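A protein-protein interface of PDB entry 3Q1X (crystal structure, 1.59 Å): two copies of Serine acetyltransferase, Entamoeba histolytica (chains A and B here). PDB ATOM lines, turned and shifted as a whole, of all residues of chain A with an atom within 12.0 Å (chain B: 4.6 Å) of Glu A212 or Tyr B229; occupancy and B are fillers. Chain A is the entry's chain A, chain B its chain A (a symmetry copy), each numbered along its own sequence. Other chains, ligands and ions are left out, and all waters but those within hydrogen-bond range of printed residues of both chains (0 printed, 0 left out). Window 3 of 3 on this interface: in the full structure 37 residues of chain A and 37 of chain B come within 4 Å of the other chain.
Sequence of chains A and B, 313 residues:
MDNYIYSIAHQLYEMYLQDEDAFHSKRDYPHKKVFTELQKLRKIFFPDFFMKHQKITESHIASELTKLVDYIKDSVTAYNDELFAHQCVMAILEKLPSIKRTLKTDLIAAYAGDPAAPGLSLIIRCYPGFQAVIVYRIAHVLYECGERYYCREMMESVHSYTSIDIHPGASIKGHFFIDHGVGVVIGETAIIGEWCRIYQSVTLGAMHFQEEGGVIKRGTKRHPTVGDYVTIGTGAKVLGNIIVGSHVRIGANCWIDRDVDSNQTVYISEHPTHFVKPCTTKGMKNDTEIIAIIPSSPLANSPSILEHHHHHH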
ATOM      1  N   HIS A 208      30.582  28.633  -7.677  1.00  0.00           N
ATOM      2  CA  HIS A 208      29.748  28.947  -8.821  1.00  0.00           C
ATOM      3  C   HIS A 208      28.272  28.775  -8.515  1.00  0.00           C
ATOM      4  O   HIS A 208      27.747  27.663  -8.464  1.00  0.00           O
ATOM      5  CB  HIS A 208      30.183  28.136 -10.035  1.00  0.00           C
ATOM      6  CG  HIS A 208      31.625  28.330 -10.375  1.00  0.00           C
ATOM      7  ND1 HIS A 208      32.580  27.362 -10.150  1.00  0.00           N
ATOM      8  CD2 HIS A 208      32.285  29.404 -10.865  1.00  0.00           C
ATOM      9  CE1 HIS A 208      33.763  27.824 -10.513  1.00  0.00           C
ATOM     10  NE2 HIS A 208      33.612  29.060 -10.953  1.00  0.00           N
ATOM     11  N   PHE A 209      27.617  29.905  -8.290  1.00  0.00           N
ATOM     12  CA  PHE A 209      26.182  29.910  -8.066  1.00  0.00           C
ATOM     13  C   PHE A 209      25.465  29.608  -9.367  1.00  0.00           C
ATOM     14  O   PHE A 209      25.801  30.156 -10.426  1.00  0.00           O
ATOM     15  CB  PHE A 209      25.732  31.238  -7.466  1.00  0.00           C
ATOM     16  CG  PHE A 209      26.331  31.515  -6.124  1.00  0.00           C
ATOM     17  CD1 PHE A 209      25.946  30.774  -5.011  1.00  0.00           C
ATOM     18  CD2 PHE A 209      27.299  32.500  -5.971  1.00  0.00           C
ATOM     19  CE1 PHE A 209      26.503  31.022  -3.762  1.00  0.00           C
ATOM     20  CE2 PHE A 209      27.865  32.756  -4.727  1.00  0.00           C
ATOM     21  CZ  PHE A 209      27.462  32.018  -3.618  1.00  0.00           C
ATOM     22  N   GLN A 210      24.485  28.715  -9.276  1.00  0.00           N
ATOM     23  CA  GLN A 210      23.815  28.196 -10.453  1.00  0.00           C
ATOM     24  C   GLN A 210      23.188  29.294 -11.299  1.00  0.00           C
ATOM     25  O   GLN A 210      22.351  30.068 -10.825  1.00  0.00           O
ATOM     26  CB  GLN A 210      22.763  27.160 -10.067  1.00  0.00           C
ATOM     27  CG  GLN A 210      23.347  25.840  -9.620  1.00  0.00           C
ATOM     28  CD  GLN A 210      22.280  24.863  -9.194  1.00  0.00           C
ATOM     29  OE1 GLN A 210      21.397  24.508  -9.981  1.00  0.00           O
ATOM     30  NE2 GLN A 210      22.352  24.419  -7.942  1.00  0.00           N
ATOM     31  N   GLU A 211      23.650  29.371 -12.539  1.00  0.00           N
ATOM     32  CA  GLU A 211      22.977  30.120 -13.576  1.00  0.00           C
ATOM     33  C   GLU A 211      22.279  29.067 -14.409  1.00  0.00           C
ATOM     34  O   GLU A 211      22.917  28.401 -15.226  1.00  0.00           O
ATOM     35  CB  GLU A 211      23.985  30.895 -14.415  1.00  0.00           C
ATOM     36  N   GLU A 212      20.986  28.863 -14.163  1.00  0.00           N
ATOM     37  CA  GLU A 212      20.206  27.953 -15.007  1.00  0.00           C
ATOM     38  C   GLU A 212      19.331  28.715 -16.018  1.00  0.00           C
ATOM     39  O   GLU A 212      18.294  29.279 -15.653  1.00  0.00           O
ATOM     40  CB  GLU A 212      19.389  26.932 -14.187  1.00  0.00           C
ATOM     41  CG  GLU A 212      18.554  25.930 -15.042  1.00  0.00           C
ATOM     42  CD  GLU A 212      19.136  24.498 -15.156  1.00  0.00           C
ATOM     43  OE1 GLU A 212      20.366  24.284 -14.991  1.00  0.00           O
ATOM     44  OE2 GLU A 212      18.332  23.566 -15.422  1.00  0.00           O
ATOM     45  N   GLY A 213      19.758  28.765 -17.281  1.00  0.00           N
ATOM     46  CA  GLY A 213      21.078  28.300 -17.728  1.00  0.00           C
ATOM     47  C   GLY A 213      21.399  26.829 -17.512  1.00  0.00           C
ATOM     48  O   GLY A 213      20.496  25.998 -17.344  1.00  0.00           O
ATOM     49  N   GLY A 214      22.694  26.517 -17.516  1.00  0.00           N
ATOM     50  CA  GLY A 214      23.164  25.150 -17.321  1.00  0.00           C
ATOM     51  C   GLY A 214      24.669  24.992 -17.190  1.00  0.00           C
ATOM     52  O   GLY A 214      25.166  24.715 -16.094  1.00  0.00           O
ATOM     53  N   VAL A 215      25.394  25.198 -18.293  1.00  0.00           N
ATOM     54  CA  VAL A 215      26.797  24.751 -18.413  1.00  0.00           C
ATOM     55  C   VAL A 215      27.862  25.860 -18.328  1.00  0.00           C
ATOM     56  O   VAL A 215      28.030  26.660 -19.261  1.00  0.00           O
ATOM     57  CB  VAL A 215      27.022  23.924 -19.707  1.00  0.00           C
ATOM     58  CG1 VAL A 215      28.353  23.192 -19.638  1.00  0.00           C
ATOM     59  CG2 VAL A 215      25.876  22.933 -19.932  1.00  0.00           C
ATOM     60  N   ILE A 216      28.609  25.869 -17.227  1.00  0.00           N
ATOM     61  CA  ILE A 216      29.554  26.956 -16.952  1.00  0.00           C
ATOM     62  C   ILE A 216      30.731  26.966 -17.919  1.00  0.00           C
ATOM     63  O   ILE A 216      31.155  25.912 -18.402  1.00  0.00           O
ATOM     64  CB  ILE A 216      30.072  26.930 -15.493  1.00  0.00           C
ATOM     65  CG1 ILE A 216      28.899  26.962 -14.513  1.00  0.00           C
ATOM     66  CG2 ILE A 216      30.990  28.132 -15.221  1.00  0.00           C
ATOM     67  CD1 ILE A 216      29.232  26.425 -13.143  1.00  0.00           C
ATOM     68  N   LYS A 217      31.221  28.174 -18.210  1.00  0.00           N
ATOM     69  CA  LYS A 217      32.396  28.398 -19.051  1.00  0.00           C
ATOM     70  C   LYS A 217      33.555  27.537 -18.577  1.00  0.00           C
ATOM     71  O   LYS A 217      33.775  27.398 -17.376  1.00  0.00           O
ATOM     72  CB  LYS A 217      32.801  29.878 -18.994  1.00  0.00           C
ATOM     73  CG  LYS A 217      34.029  30.243 -19.844  1.00  0.00           C
ATOM     74  CD  LYS A 217      34.283  31.755 -19.881  1.00  0.00           C
ATOM     75  CE  LYS A 217      34.784  32.292 -18.549  1.00  0.00           C
ATOM     76  NZ  LYS A 217      35.867  31.415 -18.017  1.00  0.00           N
ATOM     77  N   ARG A 218      34.285  26.950 -19.519  1.00  0.00           N
ATOM     78  CA  ARG A 218      35.420  26.113 -19.152  1.00  0.00           C
ATOM     79  C   ARG A 218      36.639  26.967 -18.879  1.00  0.00           C
ATOM     80  O   ARG A 218      36.940  27.895 -19.632  1.00  0.00           O
ATOM     81  CB  ARG A 218      35.713  25.066 -20.229  1.00  0.00           C
ATOM     82  CG  ARG A 218      34.459  24.385 -20.764  1.00  0.00           C
ATOM     83  CD  ARG A 218      33.411  24.205 -19.665  1.00  0.00           C
ATOM     84  NE  ARG A 218      33.572  22.947 -18.974  1.00  0.00           N
ATOM     85  CZ  ARG A 218      32.804  22.514 -17.978  1.00  0.00           C
ATOM     86  NH1 ARG A 218      31.787  23.237 -17.504  1.00  0.00           N
ATOM     87  NH2 ARG A 218      33.073  21.342 -17.449  1.00  0.00           N
ATOM     88  N   GLU B 194      16.372  18.444  -6.567  1.00  0.00           N
ATOM     89  CA  GLU B 194      17.109  18.338  -7.819  1.00  0.00           C
ATOM     90  C   GLU B 194      18.097  19.492  -7.955  1.00  0.00           C
ATOM     91  O   GLU B 194      17.872  20.571  -7.402  1.00  0.00           O
ATOM     92  CB  GLU B 194      16.115  18.376  -8.995  1.00  0.00           C
ATOM     93  CG  GLU B 194      16.611  17.787 -10.308  1.00  0.00           C
ATOM     94  CD  GLU B 194      16.489  16.272 -10.375  1.00  0.00           C
ATOM     95  OE1 GLU B 194      17.070  15.676 -11.305  1.00  0.00           O
ATOM     96  OE2 GLU B 194      15.820  15.673  -9.501  1.00  0.00           O
ATOM     97  N   TRP B 195      19.179  19.270  -8.701  1.00  0.00           N
ATOM     98  CA  TRP B 195      20.135  20.329  -9.021  1.00  0.00           C
ATOM     99  C   TRP B 195      20.716  21.022  -7.792  1.00  0.00           C
ATOM    100  O   TRP B 195      20.748  22.252  -7.708  1.00  0.00           O
ATOM    101  CB  TRP B 195      19.514  21.351  -9.989  1.00  0.00           C
ATOM    102  CG  TRP B 195      19.593  20.929 -11.403  1.00  0.00           C
ATOM    103  CD1 TRP B 195      18.571  20.484 -12.183  1.00  0.00           C
ATOM    104  CD2 TRP B 195      20.763  20.927 -12.224  1.00  0.00           C
ATOM    105  NE1 TRP B 195      19.030  20.202 -13.450  1.00  0.00           N
ATOM    106  CE2 TRP B 195      20.375  20.466 -13.501  1.00  0.00           C
ATOM    107  CE3 TRP B 195      22.107  21.272 -12.003  1.00  0.00           C
ATOM    108  CZ2 TRP B 195      21.285  20.330 -14.558  1.00  0.00           C
ATOM    109  CZ3 TRP B 195      23.015  21.136 -13.056  1.00  0.00           C
ATOM    110  CH2 TRP B 195      22.595  20.671 -14.316  1.00  0.00           C
ATOM    111  N   GLY B 227      15.299  22.564  -1.241  1.00  0.00           N
ATOM    112  CA  GLY B 227      14.539  22.507  -2.498  1.00  0.00           C
ATOM    113  C   GLY B 227      15.412  22.268  -3.716  1.00  0.00           C
ATOM    114  O   GLY B 227      16.481  21.650  -3.618  1.00  0.00           O
ATOM    115  N   ASP B 228      14.950  22.753  -4.868  1.00  0.00           N
ATOM    116  CA  ASP B 228      15.640  22.562  -6.145  1.00  0.00           C
ATOM    117  C   ASP B 228      16.520  23.756  -6.495  1.00  0.00           C
ATOM    118  O   ASP B 228      16.264  24.878  -6.055  1.00  0.00           O
ATOM    119  CB  ASP B 228      14.622  22.324  -7.265  1.00  0.00           C
ATOM    120  CG  ASP B 228      13.693  21.156  -6.979  1.00  0.00           C
ATOM    121  OD1 ASP B 228      14.116  20.191  -6.311  1.00  0.00           O
ATOM    122  OD2 ASP B 228      12.534  21.193  -7.441  1.00  0.00           O
ATOM    123  N   TYR B 229      17.572  23.509  -7.271  1.00  0.00           N
ATOM    124  CA  TYR B 229      18.465  24.571  -7.743  1.00  0.00           C
ATOM    125  C   TYR B 229      19.082  25.393  -6.604  1.00  0.00           C
ATOM    126  O   TYR B 229      19.138  26.630  -6.662  1.00  0.00           O
ATOM    127  CB  TYR B 229      17.737  25.473  -8.740  1.00  0.00           C
ATOM    128  CG  TYR B 229      17.324  24.754  -9.997  1.00  0.00           C
ATOM    129  CD1 TYR B 229      18.217  24.605 -11.052  1.00  0.00           C
ATOM    130  CD2 TYR B 229      16.043  24.210 -10.127  1.00  0.00           C
ATOM    131  CE1 TYR B 229      17.853  23.936 -12.206  1.00  0.00           C
ATOM    132  CE2 TYR B 229      15.665  23.538 -11.285  1.00  0.00           C
ATOM    133  CZ  TYR B 229      16.578  23.409 -12.321  1.00  0.00           C
ATOM    134  OH  TYR B 229      16.221  22.751 -13.477  1.00  0.00           O
ATOM    135  N   VAL B 230      19.540  24.690  -5.574  1.00  0.00           N
ATOM    136  CA  VAL B 230      20.194  25.310  -4.436  1.00  0.00           C
ATOM    137  C   VAL B 230      21.697  25.129  -4.557  1.00  0.00           C
ATOM    138  O   VAL B 230      22.174  24.040  -4.903  1.00  0.00           O
ATOM    139  CB  VAL B 230      19.695  24.700  -3.110  1.00  0.00           C
ATOM    140  CG1 VAL B 230      20.495  25.216  -1.909  1.00  0.00           C
ATOM    141  CG2 VAL B 230      18.206  24.969  -2.941  1.00  0.00           C
ATOM    142  N   THR B 231      22.431  26.204  -4.293  1.00  0.00           N
ATOM    143  CA  THR B 231      23.892  26.151  -4.237  1.00  0.00           C
ATOM    144  C   THR B 231      24.360  26.505  -2.835  1.00  0.00           C
ATOM    145  O   THR B 231      24.001  27.558  -2.293  1.00  0.00           O
ATOM    146  CB  THR B 231      24.544  27.086  -5.276  1.00  0.00           C
ATOM    147  OG1 THR B 231      23.933  26.870  -6.548  1.00  0.00           O
ATOM    148  CG2 THR B 231      26.047  26.818  -5.390  1.00  0.00           C
ATOM    149  N   HIS B 247      15.922  27.583  -5.634  1.00  0.00           N
ATOM    150  CA  HIS B 247      16.669  28.713  -6.197  1.00  0.00           C
ATOM    151  C   HIS B 247      17.278  29.601  -5.099  1.00  0.00           C
ATOM    152  O   HIS B 247      17.143  30.828  -5.116  1.00  0.00           O
ATOM    153  CB  HIS B 247      15.793  29.518  -7.177  1.00  0.00           C
ATOM    154  CG  HIS B 247      15.305  28.720  -8.348  1.00  0.00           C
ATOM    155  ND1 HIS B 247      14.071  28.100  -8.368  1.00  0.00           N
ATOM    156  CD2 HIS B 247      15.882  28.442  -9.541  1.00  0.00           C
ATOM    157  CE1 HIS B 247      13.915  27.471  -9.519  1.00  0.00           C
ATOM    158  NE2 HIS B 247      14.999  27.662 -10.249  1.00  0.00           N
ATOM    159  N   VAL B 248      17.936  28.954  -4.139  1.00  0.00           N
ATOM    160  CA  VAL B 248      18.615  29.635  -3.045  1.00  0.00           C
ATOM    161  C   VAL B 248      20.130  29.536  -3.241  1.00  0.00           C
ATOM    162  O   VAL B 248      20.653  28.476  -3.583  1.00  0.00           O
ATOM    163  CB  VAL B 248      18.200  29.044  -1.665  1.00  0.00           C
ATOM    164  CG1 VAL B 248      19.084  29.570  -0.550  1.00  0.00           C
ATOM    165  CG2 VAL B 248      16.731  29.357  -1.365  1.00  0.00           C
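CG2 of Thr B231 touches O of His A208 (3.6 Å).
Phe A209 touches Thr B231.
Gln A210 touches Tyr B229 (OE1 to CD1, 3.4 Å).
Glu A212 touches Trp B195.
Of the 11 printed residues of chain A, 4 touch a printed residue of chain B.
Hydrophobic or aromatic side chains of chain A within 4 Å of the printed part of chain B: Phe A209.
Hydrophobic or aromatic side chains of chain B within 4 Å of the printed part of chain A: Trp B195 and Tyr B229.
Among the printed residues, 8 pairs touch across the chains.
Among the printed residues, no Asp or Glu carboxylate lies within 4 Å of a Lys or Arg side-chain nitrogen of the other chain.
The backbone NH (N) of Thr B231 is in hydrogen-bond range of the backbone carbonyl oxygen (O) of Val B248 (3.0 Å).
The backbone NH (N) of Val B230 sits at hydrogen-bond distance from the backbone carbonyl oxygen (O) of Trp B195, at 3.5 Å.
The backbone carbonyl oxygen (O) of Trp B195 lies close to the backbone NH (N) of Tyr B229 (3.4 Å).
N of Tyr B229 is in hydrogen-bond range of O of Glu B194 (3.0 Å).
Of the printed residues of chain B, His A208 touches Thr B231.
Printed residues of chain B within 4 Å of Phe A209: Thr B231.
Printed residues of chain B within 4 Å of Gln A210: Trp B195, Tyr B229, Val B230 and Thr B231.
Of chain B, only Trp B195 (3.96 Å) and Tyr B229 (3.0 Å) come within 4 Å of Glu A212.
Arg A218 touches none of the printed residues of chain B.
Trp B195 touches just these residues of chain A: Gln A210 and Glu A212.
No residue of chain A comes within 4 Å of Gly B227.
Val B230 touches just one residue of chain A: Gln A210.
Of chain A, only His A208 (3.6 Å), Phe A209 (3.95 Å) and Gln A210 (3.2 Å) come within 4 Å of Thr B231.
No residue of chain A comes within 4 Å of His B247.
Val B248 touches none of the printed residues of chain A.
The nearest printed residue of chain B that does not touch His A208 is Val B230 (7.5 Å).
No position is printed for both chains.
OE2 of Glu A212 is in hydrogen-bond range of OH of Tyr B229 (3.0 Å).
The side-chain amide nitrogen (NE2) of Gln A210 sits at hydrogen-bond distance from the side-chain hydroxyl (OG1) of Thr B231.
The side-chain amide nitrogen (NE2) of Gln A210 is in hydrogen-bond range of the backbone carbonyl oxygen (O) of Val B230 (3.1 Å).
O of Trp B195 is in hydrogen-bond range of NE2 of Gln A210, 2.7 Å away.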
